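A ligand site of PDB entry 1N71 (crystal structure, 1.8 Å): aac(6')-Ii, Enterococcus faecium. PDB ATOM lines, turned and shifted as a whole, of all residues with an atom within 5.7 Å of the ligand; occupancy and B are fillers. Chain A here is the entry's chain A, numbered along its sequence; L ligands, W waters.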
ATOM      1  N   THR A  24      24.166  17.066  23.787  1.00  0.00           N
ATOM      2  CA  THR A  24      23.644  17.841  22.668  1.00  0.00           C
ATOM      3  C   THR A  24      24.391  17.606  21.367  1.00  0.00           C
ATOM      4  O   THR A  24      23.782  17.309  20.331  1.00  0.00           O
ATOM      5  CB  THR A  24      23.664  19.349  22.992  1.00  0.00           C
ATOM      6  OG1 THR A  24      22.945  19.594  24.213  1.00  0.00           O
ATOM      7  CG2 THR A  24      23.014  20.145  21.868  1.00  0.00           C
ATOM      8  N   TRP A  25      25.713  17.751  21.412  1.00  0.00           N
ATOM      9  CA  TRP A  25      26.552  17.567  20.228  1.00  0.00           C
ATOM     10  C   TRP A  25      27.628  16.517  20.515  1.00  0.00           C
ATOM     11  O   TRP A  25      28.790  16.854  20.738  1.00  0.00           O
ATOM     12  CB  TRP A  25      27.217  18.888  19.839  1.00  0.00           C
ATOM     13  CG  TRP A  25      26.266  19.919  19.323  1.00  0.00           C
ATOM     14  CD1 TRP A  25      25.604  19.904  18.130  1.00  0.00           C
ATOM     15  CD2 TRP A  25      25.879  21.139  19.975  1.00  0.00           C
ATOM     16  NE1 TRP A  25      24.827  21.025  17.997  1.00  0.00           N
ATOM     17  CE2 TRP A  25      24.976  21.801  19.116  1.00  0.00           C
ATOM     18  CE3 TRP A  25      26.198  21.729  21.205  1.00  0.00           C
ATOM     19  CZ2 TRP A  25      24.397  23.035  19.451  1.00  0.00           C
ATOM     20  CZ3 TRP A  25      25.628  22.955  21.533  1.00  0.00           C
ATOM     21  CH2 TRP A  25      24.735  23.597  20.650  1.00  0.00           C
ATOM     22  N   LEU A  76      25.455  28.193  22.185  1.00  0.00           N
ATOM     23  CA  LEU A  76      24.163  28.451  22.812  1.00  0.00           C
ATOM     24  C   LEU A  76      23.500  27.088  22.915  1.00  0.00           C
ATOM     25  O   LEU A  76      23.203  26.454  21.892  1.00  0.00           O
ATOM     26  CB  LEU A  76      23.282  29.387  21.976  1.00  0.00           C
ATOM     27  CG  LEU A  76      21.867  29.534  22.546  1.00  0.00           C
ATOM     28  CD1 LEU A  76      21.921  29.962  24.024  1.00  0.00           C
ATOM     29  CD2 LEU A  76      21.070  30.546  21.734  1.00  0.00           C
ATOM     30  N   VAL A  77      23.278  26.631  24.137  1.00  0.00           N
ATOM     31  CA  VAL A  77      22.647  25.350  24.335  1.00  0.00           C
ATOM     32  C   VAL A  77      21.720  25.387  25.533  1.00  0.00           C
ATOM     33  O   VAL A  77      22.034  25.996  26.566  1.00  0.00           O
ATOM     34  CB  VAL A  77      23.703  24.236  24.558  1.00  0.00           C
ATOM     35  CG1 VAL A  77      24.548  24.566  25.774  1.00  0.00           C
ATOM     36  CG2 VAL A  77      23.015  22.883  24.737  1.00  0.00           C
ATOM     37  N   VAL A  78      20.576  24.739  25.380  1.00  0.00           N
ATOM     38  CA  VAL A  78      19.567  24.642  26.420  1.00  0.00           C
ATOM     39  C   VAL A  78      19.213  23.169  26.502  1.00  0.00           C
ATOM     40  O   VAL A  78      19.023  22.529  25.465  1.00  0.00           O
ATOM     41  CB  VAL A  78      18.291  25.436  26.039  1.00  0.00           C
ATOM     42  CG1 VAL A  78      17.196  25.204  27.081  1.00  0.00           C
ATOM     43  CG2 VAL A  78      18.624  26.924  25.939  1.00  0.00           C
ATOM     44  N   GLU A  79      19.153  22.601  27.708  1.00  0.00           N
ATOM     45  CA  GLU A  79      18.810  21.186  27.831  1.00  0.00           C
ATOM     46  C   GLU A  79      17.590  20.908  26.964  1.00  0.00           C
ATOM     47  O   GLU A  79      16.600  21.635  27.022  1.00  0.00           O
ATOM     48  CB  GLU A  79      18.467  20.820  29.276  1.00  0.00           C
ATOM     49  CG  GLU A  79      19.597  21.009  30.259  1.00  0.00           C
ATOM     50  CD  GLU A  79      19.283  20.390  31.604  1.00  0.00           C
ATOM     51  OE1 GLU A  79      18.184  20.660  32.139  1.00  0.00           O
ATOM     52  OE2 GLU A  79      20.133  19.662  32.137  1.00  0.00           O
ATOM     53  N   ARG A  82      14.289  21.242  28.504  1.00  0.00           N
ATOM     54  CA  ARG A  82      13.862  22.501  29.104  1.00  0.00           C
ATOM     55  C   ARG A  82      13.632  23.598  28.066  1.00  0.00           C
ATOM     56  O   ARG A  82      13.491  24.779  28.419  1.00  0.00           O
ATOM     57  CB  ARG A  82      14.891  22.982  30.117  1.00  0.00           C
ATOM     58  CG  ARG A  82      15.150  22.032  31.276  1.00  0.00           C
ATOM     59  CD  ARG A  82      13.865  21.714  32.035  1.00  0.00           C
ATOM     60  NE  ARG A  82      14.141  21.354  33.424  1.00  0.00           N
ATOM     61  CZ  ARG A  82      14.552  22.210  34.347  1.00  0.00           C
ATOM     62  NH1 ARG A  82      14.718  23.486  34.033  1.00  0.00           N
ATOM     63  NH2 ARG A  82      14.789  21.795  35.580  1.00  0.00           N
ATOM     64  N   ARG A  83      13.585  23.215  26.801  1.00  0.00           N
ATOM     65  CA  ARG A  83      13.399  24.163  25.715  1.00  0.00           C
ATOM     66  C   ARG A  83      11.968  24.675  25.608  1.00  0.00           C
ATOM     67  O   ARG A  83      11.048  24.150  26.235  1.00  0.00           O
ATOM     68  CB  ARG A  83      13.845  23.530  24.404  1.00  0.00           C
ATOM     69  CG  ARG A  83      15.331  23.220  24.390  1.00  0.00           C
ATOM     70  CD  ARG A  83      15.771  22.408  23.185  1.00  0.00           C
ATOM     71  NE  ARG A  83      17.193  22.114  23.258  1.00  0.00           N
ATOM     72  CZ  ARG A  83      17.829  21.262  22.441  1.00  0.00           C
ATOM     73  NH1 ARG A  83      17.172  20.630  21.496  1.00  0.00           N
ATOM     74  NH2 ARG A  83      19.129  21.065  22.596  1.00  0.00           N
ATOM     75  N   LYS A  84      11.801  25.725  24.798  1.00  0.00           N
ATOM     76  CA  LYS A  84      10.504  26.342  24.561  1.00  0.00           C
ATOM     77  C   LYS A  84       9.898  27.054  25.770  1.00  0.00           C
ATOM     78  O   LYS A  84       8.676  27.145  25.894  1.00  0.00           O
ATOM     79  CB  LYS A  84       9.522  25.312  24.024  1.00  0.00           C
ATOM     80  CG  LYS A  84       9.925  24.709  22.684  1.00  0.00           C
ATOM     81  CD  LYS A  84      10.287  25.787  21.673  1.00  0.00           C
ATOM     82  CE  LYS A  84      10.387  25.234  20.265  1.00  0.00           C
ATOM     83  NZ  LYS A  84      11.328  24.089  20.159  1.00  0.00           N
ATOM     84  N   ASN A  85      10.743  27.555  26.668  1.00  0.00           N
ATOM     85  CA  ASN A  85      10.247  28.281  27.827  1.00  0.00           C
ATOM     86  C   ASN A  85      11.097  29.524  28.119  1.00  0.00           C
ATOM     87  O   ASN A  85      11.394  29.826  29.276  1.00  0.00           O
ATOM     88  CB  ASN A  85      10.202  27.404  29.081  1.00  0.00           C
ATOM     89  CG  ASN A  85       9.512  28.089  30.254  1.00  0.00           C
ATOM     90  OD1 ASN A  85       9.638  27.666  31.398  1.00  0.00           O
ATOM     91  ND2 ASN A  85       8.781  29.167  29.974  1.00  0.00           N
ATOM     92  N   GLN A  86      11.506  30.212  27.067  1.00  0.00           N
ATOM     93  CA  GLN A  86      12.279  31.453  27.171  1.00  0.00           C
ATOM     94  C   GLN A  86      13.698  31.388  27.727  1.00  0.00           C
ATOM     95  O   GLN A  86      14.324  32.431  27.927  1.00  0.00           O
ATOM     96  CB  GLN A  86      11.489  32.483  27.979  1.00  0.00           C
ATOM     97  CG  GLN A  86      10.119  32.786  27.408  1.00  0.00           C
ATOM     98  CD  GLN A  86      10.190  33.438  26.047  1.00  0.00           C
ATOM     99  OE1 GLN A  86      10.768  34.524  25.884  1.00  0.00           O
ATOM    100  NE2 GLN A  86       9.621  32.786  25.044  1.00  0.00           N
ATOM    101  N   ILE A  87      14.215  30.195  28.003  1.00  0.00           N
ATOM    102  CA  ILE A  87      15.572  30.100  28.530  1.00  0.00           C
ATOM    103  C   ILE A  87      16.554  30.671  27.504  1.00  0.00           C
ATOM    104  O   ILE A  87      17.441  31.448  27.835  1.00  0.00           O
ATOM    105  CB  ILE A  87      15.943  28.632  28.858  1.00  0.00           C
ATOM    106  CG1 ILE A  87      15.072  28.123  30.003  1.00  0.00           C
ATOM    107  CG2 ILE A  87      17.423  28.550  29.243  1.00  0.00           C
ATOM    108  CD1 ILE A  87      15.242  26.629  30.296  1.00  0.00           C
ATOM    109  N   GLY A  88      16.384  30.267  26.245  1.00  0.00           N
ATOM    110  CA  GLY A  88      17.258  30.767  25.199  1.00  0.00           C
ATOM    111  C   GLY A  88      17.163  32.274  25.027  1.00  0.00           C
ATOM    112  O   GLY A  88      18.177  32.966  24.860  1.00  0.00           O
ATOM    113  N   THR A  89      15.947  32.795  25.078  1.00  0.00           N
ATOM    114  CA  THR A  89      15.741  34.235  24.927  1.00  0.00           C
ATOM    115  C   THR A  89      16.438  34.986  26.043  1.00  0.00           C
ATOM    116  O   THR A  89      17.153  35.963  25.804  1.00  0.00           O
ATOM    117  CB  THR A  89      14.235  34.587  24.967  1.00  0.00           C
ATOM    118  OG1 THR A  89      13.565  33.967  23.857  1.00  0.00           O
ATOM    119  CG2 THR A  89      14.044  36.096  24.898  1.00  0.00           C
ATOM    120  N   ARG A  90      16.240  34.523  27.262  1.00  0.00           N
ATOM    121  CA  ARG A  90      16.866  35.166  28.419  1.00  0.00           C
ATOM    122  C   ARG A  90      18.394  35.110  28.344  1.00  0.00           C
ATOM    123  O   ARG A  90      19.070  36.050  28.740  1.00  0.00           O
ATOM    124  CB  ARG A  90      16.328  34.524  29.692  1.00  0.00           C
ATOM    125  CG  ARG A  90      14.819  34.680  29.801  1.00  0.00           C
ATOM    126  CD  ARG A  90      14.234  33.840  30.909  1.00  0.00           C
ATOM    127  NE  ARG A  90      14.714  34.261  32.211  1.00  0.00           N
ATOM    128  CZ  ARG A  90      14.462  33.621  33.343  1.00  0.00           C
ATOM    129  NH1 ARG A  90      13.726  32.521  33.332  1.00  0.00           N
ATOM    130  NH2 ARG A  90      14.945  34.084  34.498  1.00  0.00           N
ATOM    131  N   LEU A 109      26.691  35.184  14.353  1.00  0.00           N
ATOM    132  CA  LEU A 109      26.742  33.753  14.601  1.00  0.00           C
ATOM    133  C   LEU A 109      26.578  33.004  13.291  1.00  0.00           C
ATOM    134  O   LEU A 109      26.135  33.562  12.288  1.00  0.00           O
ATOM    135  CB  LEU A 109      25.625  33.358  15.571  1.00  0.00           C
ATOM    136  CG  LEU A 109      24.213  33.696  15.066  1.00  0.00           C
ATOM    137  CD1 LEU A 109      23.668  32.545  14.224  1.00  0.00           C
ATOM    138  CD2 LEU A 109      23.299  33.975  16.250  1.00  0.00           C
ATOM    139  N   GLY A 110      26.949  31.733  13.316  1.00  0.00           N
ATOM    140  CA  GLY A 110      26.797  30.894  12.157  1.00  0.00           C
ATOM    141  C   GLY A 110      25.942  29.706  12.572  1.00  0.00           C
ATOM    142  O   GLY A 110      26.290  28.978  13.507  1.00  0.00           O
ATOM    143  N   THR A 111      24.807  29.525  11.915  1.00  0.00           N
ATOM    144  CA  THR A 111      23.922  28.403  12.210  1.00  0.00           C
ATOM    145  C   THR A 111      23.855  27.558  10.937  1.00  0.00           C
ATOM    146  O   THR A 111      23.370  28.007   9.908  1.00  0.00           O
ATOM    147  CB  THR A 111      22.510  28.880  12.636  1.00  0.00           C
ATOM    148  OG1 THR A 111      21.699  27.741  12.943  1.00  0.00           O
ATOM    149  CG2 THR A 111      21.849  29.698  11.545  1.00  0.00           C
ATOM    150  N   ASP A 112      24.367  26.333  11.018  1.00  0.00           N
ATOM    151  CA  ASP A 112      24.405  25.452   9.865  1.00  0.00           C
ATOM    152  C   ASP A 112      23.090  24.749   9.556  1.00  0.00           C
ATOM    153  O   ASP A 112      22.227  24.620  10.418  1.00  0.00           O
ATOM    154  CB  ASP A 112      25.514  24.422  10.050  1.00  0.00           C
ATOM    155  CG  ASP A 112      26.860  25.052  10.374  1.00  0.00           C
ATOM    156  OD1 ASP A 112      27.051  25.497  11.533  1.00  0.00           O
ATOM    157  OD2 ASP A 112      27.718  25.132   9.470  1.00  0.00           O
ATOM    158  N   ASN A 138      11.281  28.394   6.839  1.00  0.00           N
ATOM    159  CA  ASN A 138      11.688  27.411   7.842  1.00  0.00           C
ATOM    160  C   ASN A 138      10.943  26.105   7.624  1.00  0.00           C
ATOM    161  O   ASN A 138       9.737  26.016   7.891  1.00  0.00           O
ATOM    162  CB  ASN A 138      11.430  27.945   9.247  1.00  0.00           C
ATOM    163  CG  ASN A 138      12.223  27.201  10.310  1.00  0.00           C
ATOM    164  OD1 ASN A 138      12.839  26.167  10.020  1.00  0.00           O
ATOM    165  ND2 ASN A 138      12.198  27.713  11.535  1.00  0.00           N
ATOM    166  N   GLU A 141      11.630  23.571  11.719  1.00  0.00           N
ATOM    167  CA  GLU A 141      11.921  24.246  12.974  1.00  0.00           C
ATOM    168  C   GLU A 141      13.419  24.490  13.146  1.00  0.00           C
ATOM    169  O   GLU A 141      13.999  24.157  14.181  1.00  0.00           O
ATOM    170  CB  GLU A 141      11.386  23.447  14.159  1.00  0.00           C
ATOM    171  CG  GLU A 141       9.892  23.611  14.397  1.00  0.00           C
ATOM    172  CD  GLU A 141       9.507  23.327  15.833  1.00  0.00           C
ATOM    173  OE1 GLU A 141       9.688  22.172  16.279  1.00  0.00           O
ATOM    174  OE2 GLU A 141       9.051  24.262  16.526  1.00  0.00           O
ATOM    175  N   HIS A 142      14.039  25.070  12.121  1.00  0.00           N
ATOM    176  CA  HIS A 142      15.453  25.385  12.180  1.00  0.00           C
ATOM    177  C   HIS A 142      15.618  26.566  13.130  1.00  0.00           C
ATOM    178  O   HIS A 142      14.822  27.505  13.101  1.00  0.00           O
ATOM    179  CB  HIS A 142      15.978  25.766  10.799  1.00  0.00           C
ATOM    180  CG  HIS A 142      17.452  25.979  10.760  1.00  0.00           C
ATOM    181  ND1 HIS A 142      18.336  24.989  10.379  1.00  0.00           N
ATOM    182  CD2 HIS A 142      18.203  27.050  11.112  1.00  0.00           C
ATOM    183  CE1 HIS A 142      19.572  25.441  10.507  1.00  0.00           C
ATOM    184  NE2 HIS A 142      19.519  26.684  10.942  1.00  0.00           N
ATOM    185  N   PRO A 143      16.660  26.550  13.972  1.00  0.00           N
ATOM    186  CA  PRO A 143      16.877  27.642  14.925  1.00  0.00           C
ATOM    187  C   PRO A 143      17.176  29.031  14.373  1.00  0.00           C
ATOM    188  O   PRO A 143      17.248  29.985  15.154  1.00  0.00           O
ATOM    189  CB  PRO A 143      17.994  27.108  15.806  1.00  0.00           C
ATOM    190  CG  PRO A 143      18.803  26.281  14.847  1.00  0.00           C
ATOM    191  CD  PRO A 143      17.722  25.540  14.086  1.00  0.00           C
ATOM    192  N   TYR A 144      17.362  29.171  13.060  1.00  0.00           N
ATOM    193  CA  TYR A 144      17.649  30.508  12.539  1.00  0.00           C
ATOM    194  C   TYR A 144      16.487  31.444  12.894  1.00  0.00           C
ATOM    195  O   TYR A 144      16.690  32.612  13.189  1.00  0.00           O
ATOM    196  CB  TYR A 144      17.848  30.501  11.011  1.00  0.00           C
ATOM    197  CG  TYR A 144      16.561  30.577  10.199  1.00  0.00           C
ATOM    198  CD1 TYR A 144      15.871  29.424   9.841  1.00  0.00           C
ATOM    199  CD2 TYR A 144      16.042  31.815   9.795  1.00  0.00           C
ATOM    200  CE1 TYR A 144      14.689  29.488   9.101  1.00  0.00           C
ATOM    201  CE2 TYR A 144      14.866  31.887   9.054  1.00  0.00           C
ATOM    202  CZ  TYR A 144      14.188  30.725   8.712  1.00  0.00           C
ATOM    203  OH  TYR A 144      13.011  30.786   7.985  1.00  0.00           O
ATOM    204  N   GLU A 145      15.273  30.891  12.849  1.00  0.00           N
ATOM    205  CA  GLU A 145      14.078  31.662  13.152  1.00  0.00           C
ATOM    206  C   GLU A 145      14.060  32.105  14.608  1.00  0.00           C
ATOM    207  O   GLU A 145      13.463  33.139  14.945  1.00  0.00           O
ATOM    208  CB  GLU A 145      12.840  30.824  12.832  1.00  0.00           C
ATOM    209  CG  GLU A 145      11.515  31.546  12.986  1.00  0.00           C
ATOM    210  CD  GLU A 145      10.416  30.915  12.152  1.00  0.00           C
ATOM    211  OE1 GLU A 145      10.367  29.668  12.096  1.00  0.00           O
ATOM    212  OE2 GLU A 145       9.601  31.663  11.570  1.00  0.00           O
ATOM    213  N   PHE A 146      14.701  31.339  15.468  1.00  0.00           N
ATOM    214  CA  PHE A 146      14.790  31.687  16.880  1.00  0.00           C
ATOM    215  C   PHE A 146      15.559  33.005  16.974  1.00  0.00           C
ATOM    216  O   PHE A 146      15.146  33.945  17.667  1.00  0.00           O
ATOM    217  CB  PHE A 146      15.549  30.602  17.657  1.00  0.00           C
ATOM    218  CG  PHE A 146      16.099  31.059  18.978  1.00  0.00           C
ATOM    219  CD1 PHE A 146      15.255  31.317  20.058  1.00  0.00           C
ATOM    220  CD2 PHE A 146      17.469  31.249  19.141  1.00  0.00           C
ATOM    221  CE1 PHE A 146      15.777  31.766  21.279  1.00  0.00           C
ATOM    222  CE2 PHE A 146      18.003  31.688  20.347  1.00  0.00           C
ATOM    223  CZ  PHE A 146      17.151  31.951  21.423  1.00  0.00           C
ATOM    224  N   TYR A 147      16.673  33.077  16.253  1.00  0.00           N
ATOM    225  CA  TYR A 147      17.486  34.283  16.268  1.00  0.00           C
ATOM    226  C   TYR A 147      16.764  35.446  15.598  1.00  0.00           C
ATOM    227  O   TYR A 147      16.838  36.584  16.079  1.00  0.00           O
ATOM    228  CB  TYR A 147      18.829  34.008  15.585  1.00  0.00           C
ATOM    229  CG  TYR A 147      19.690  33.047  16.368  1.00  0.00           C
ATOM    230  CD1 TYR A 147      20.261  33.421  17.588  1.00  0.00           C
ATOM    231  CD2 TYR A 147      19.911  31.750  15.905  1.00  0.00           C
ATOM    232  CE1 TYR A 147      21.031  32.527  18.332  1.00  0.00           C
ATOM    233  CE2 TYR A 147      20.690  30.849  16.643  1.00  0.00           C
ATOM    234  CZ  TYR A 147      21.248  31.244  17.843  1.00  0.00           C
ATOM    235  OH  TYR A 147      22.013  30.365  18.561  1.00  0.00           O
ATOM    236  N   LYS A 149      13.680  36.124  15.614  1.00  0.00           N
ATOM    237  CA  LYS A 149      12.743  36.671  16.578  1.00  0.00           C
ATOM    238  C   LYS A 149      13.428  37.504  17.650  1.00  0.00           C
ATOM    239  O   LYS A 149      12.791  38.311  18.329  1.00  0.00           O
ATOM    240  CB  LYS A 149      11.913  35.551  17.204  1.00  0.00           C
ATOM    241  CG  LYS A 149      10.955  34.904  16.197  1.00  0.00           C
ATOM    242  CD  LYS A 149       9.971  33.964  16.847  1.00  0.00           C
ATOM    243  CE  LYS A 149       8.984  33.414  15.830  1.00  0.00           C
ATOM    244  NZ  LYS A 149       7.986  32.509  16.478  1.00  0.00           N
HETATM  245  N1  LIG L   1      12.527  27.180  15.143  1.00  0.00           N
HETATM  246  C1  LIG L   1      11.675  28.213  15.129  1.00  0.00           C
HETATM  247  N2  LIG L   1      11.347  29.032  16.149  1.00  0.00           N
HETATM  248  C2  LIG L   1      12.028  28.703  17.294  1.00  0.00           C
HETATM  249  C3  LIG L   1      12.933  27.676  17.468  1.00  0.00           C
HETATM  250  C4  LIG L   1      13.192  26.878  16.309  1.00  0.00           C
HETATM  251  N3  LIG L   1      14.048  25.855  16.332  1.00  0.00           N
HETATM  252  N4  LIG L   1      13.419  27.654  18.764  1.00  0.00           N
HETATM  253  C5  LIG L   1      12.802  28.641  19.340  1.00  0.00           C
HETATM  254  N5  LIG L   1      11.939  29.325  18.518  1.00  0.00           N
HETATM  255  C6  LIG L   1      11.076  30.473  18.844  1.00  0.00           C
HETATM  256  C7  LIG L   1       9.971  30.133  19.846  1.00  0.00           C
HETATM  257  O1  LIG L   1       8.829  29.641  19.136  1.00  0.00           O
HETATM  258  C8  LIG L   1       9.607  31.461  20.509  1.00  0.00           C
HETATM  259  O2  LIG L   1       8.788  32.207  19.598  1.00  0.00           O
HETATM  260  P1  LIG L   1       7.379  32.835  20.062  1.00  0.00           P
HETATM  261  O3  LIG L   1       6.593  31.659  20.522  1.00  0.00           O
HETATM  262  O4  LIG L   1       6.854  33.467  18.829  1.00  0.00           O
HETATM  263  O5  LIG L   1       7.733  33.792  21.136  1.00  0.00           O
HETATM  264  C9  LIG L   1      10.984  32.142  20.574  1.00  0.00           C
HETATM  265  O6  LIG L   1      11.743  31.536  19.527  1.00  0.00           O
HETATM  266  C10 LIG L   1      11.701  32.023  21.931  1.00  0.00           C
HETATM  267  O7  LIG L   1      12.124  30.674  22.158  1.00  0.00           O
HETATM  268  P2  LIG L   1      12.817  30.210  23.530  1.00  0.00           P
HETATM  269  O8  LIG L   1      11.830  29.443  24.327  1.00  0.00           O
HETATM  270  O9  LIG L   1      13.521  31.367  24.135  1.00  0.00           O
HETATM  271  O10 LIG L   1      13.920  29.195  22.967  1.00  0.00           O
HETATM  272  P3  LIG L   1      14.632  27.969  23.735  1.00  0.00           P
HETATM  273  O11 LIG L   1      13.962  26.710  23.333  1.00  0.00           O
HETATM  274  O12 LIG L   1      14.796  28.285  25.163  1.00  0.00           O
HETATM  275  O13 LIG L   1      16.083  27.989  23.059  1.00  0.00           O
HETATM  276  C11 LIG L   1      17.375  27.174  21.159  1.00  0.00           C
HETATM  277  C12 LIG L   1      16.227  28.054  21.627  1.00  0.00           C
HETATM  278  C13 LIG L   1      17.421  27.207  19.624  1.00  0.00           C
HETATM  279  C14 LIG L   1      18.709  27.727  21.743  1.00  0.00           C
HETATM  280  C15 LIG L   1      17.111  25.695  21.688  1.00  0.00           C
HETATM  281  O14 LIG L   1      15.908  25.144  21.137  1.00  0.00           O
HETATM  282  C16 LIG L   1      18.318  24.759  21.504  1.00  0.00           C
HETATM  283  O15 LIG L   1      19.048  24.496  22.464  1.00  0.00           O
HETATM  284  N6  LIG L   1      18.509  24.272  20.272  1.00  0.00           N
HETATM  285  C17 LIG L   1      19.591  23.381  19.875  1.00  0.00           C
HETATM  286  C18 LIG L   1      20.934  24.089  19.734  1.00  0.00           C
HETATM  287  C19 LIG L   1      21.088  24.832  18.424  1.00  0.00           C
HETATM  288  O16 LIG L   1      20.866  24.264  17.340  1.00  0.00           O
HETATM  289  N7  LIG L   1      21.478  26.110  18.506  1.00  0.00           N
HETATM  290  C20 LIG L   1      21.690  27.018  17.371  1.00  0.00           C
HETATM  291  C21 LIG L   1      23.071  27.644  17.398  1.00  0.00           C
HETATM  292  S1  LIG L   1      23.895  27.625  15.799  1.00  0.00           S
HETATM  293  O   HOH W   1       9.039  30.289  15.689  1.00  0.00           O
HETATM  294  O   HOH W   2       9.778  34.766  22.763  1.00  0.00           O
HETATM  295  O   HOH W   3      12.076  35.242  21.935  1.00  0.00           O
HETATM  296  O   HOH W   4       9.225  30.143  24.246  1.00  0.00           O
HETATM  297  O   HOH W   5       7.705  29.350  22.199  1.00  0.00           O
HETATM  298  O   HOH W   6      13.388  27.420  27.309  1.00  0.00           O
HETATM  299  O   HOH W   7      13.318  25.650  20.938  1.00  0.00           O
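The backbone NH of Thr 89 is in hydrogen-bond range of an oxygen (O9) of the ligand (3.0 Å).
An oxygen (O9) of the ligand is in hydrogen-bond range of the side-chain hydroxyl of Thr 89 (2.6 Å).
A nitrogen (N3) of the ligand is in hydrogen-bond range of the backbone carbonyl oxygen of Glu 141.
The backbone NH (N) of Gly 88 lies within hydrogen-bond range of an oxygen (O12) of the ligand (2.8 Å).
The side-chain amino group (NZ) of Lys 149 lies within salt-bridge range of an oxygen (O4) of the ligand, 2.8 Å away.
An oxygen (O11) of the ligand lies within hydrogen-bond range of the backbone NH of Lys 84 (2.8 Å).
An oxygen (O8) of the ligand lies within hydrogen-bond range of the backbone NH (N) of Gln 86 (2.9 Å).
An oxygen (O15) of the ligand is in hydrogen-bond range of the guanidinium group (NE) of Arg 83 (3.1 Å).
O8 of the ligand sits at hydrogen-bond distance from N of Asn 85, at 3.2 Å.
N of Val 78 sits at hydrogen-bond distance from O15 of the ligand (3.3 Å).
N of Ile 87 is in hydrogen-bond range of O12 of the ligand, 3.5 Å away.
The backbone carbonyl oxygen (O) of Gly 110 sits close to a sulfur (S1) of the ligand.
A sulfur (S1) of the ligand lies close to the side-chain hydroxyl (OG1) of Thr 111, 3.6 Å away.
N1 of the ligand lies close to O of His 142, 3.1 Å away.
CZ2 of Trp 25 touches C18 of the ligand, 3.6 Å away.
Leu 76 touches the ligand.
ND2 of Asn 138 touches N1 of the ligand, at 3.7 Å.
Pro 143 touches the ligand (N to N3, 3.6 Å).
Glu 145 touches the ligand.
Phe 146 touches the ligand (CD1 to O6, 3.6 Å).
Tyr 147 touches the ligand (OH to C21, 3.1 Å).
Within 4 Å of the ligand: Trp 25, Leu 76, Val 78, Arg 83, Lys 84, Asn 85, Gln 86, Ile 87, Gly 88, Thr 89, Gly 110, Thr 111, Asn 138, Glu 141, His 142, Pro 143, Glu 145, Phe 146, Tyr 147 and Lys 149.
The side-chain hydroxyl of Thr 89 lies within hydrogen-bond range of the side-chain amide oxygen of Gln 86 (3.5 Å).
N of Glu 141 sits at hydrogen-bond distance from OD1 of Asn 138 (3.3 Å).
A ring nitrogen (NE2) of His 142 is in hydrogen-bond range of the side-chain hydroxyl (OG1) of Thr 111 (3.1 Å).
OD1 of Asn 138 is in hydrogen-bond range of N of His 142 (2.7 Å).
O of Asp 112 sits close to NE2 of His 142, at 3.4 Å.
The guanidinium group (NE) of Arg 83 is in hydrogen-bond range of the backbone carbonyl oxygen (O) of Val 78 (2.9 Å).
The side-chain carboxylate of Glu 145 is in hydrogen-bond range of the side-chain amide nitrogen of Asn 138, 2.7 Å away.
N of Asn 138 is in hydrogen-bond range of OH of Tyr 144 (3.2 Å).
Water W7 bridges the side-chain amino group (NZ) of Lys 84 and an oxygen (O14) of the ligand.
Water W1 lies within hydrogen-bond range of NZ of Lys 149 (2.6 Å) and N2 of the ligand (2.7 Å).
Water W4 lies within hydrogen-bond range of an oxygen (O8) of the ligand (2.7 Å), the side-chain amide nitrogen of Gln 86 (2.8 Å) and the backbone carbonyl oxygen of Lys 84 (3.5 Å).
Water W2 bridges O5 of the ligand (2.8 Å) and NE2 of Gln 86 (3.0 Å).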
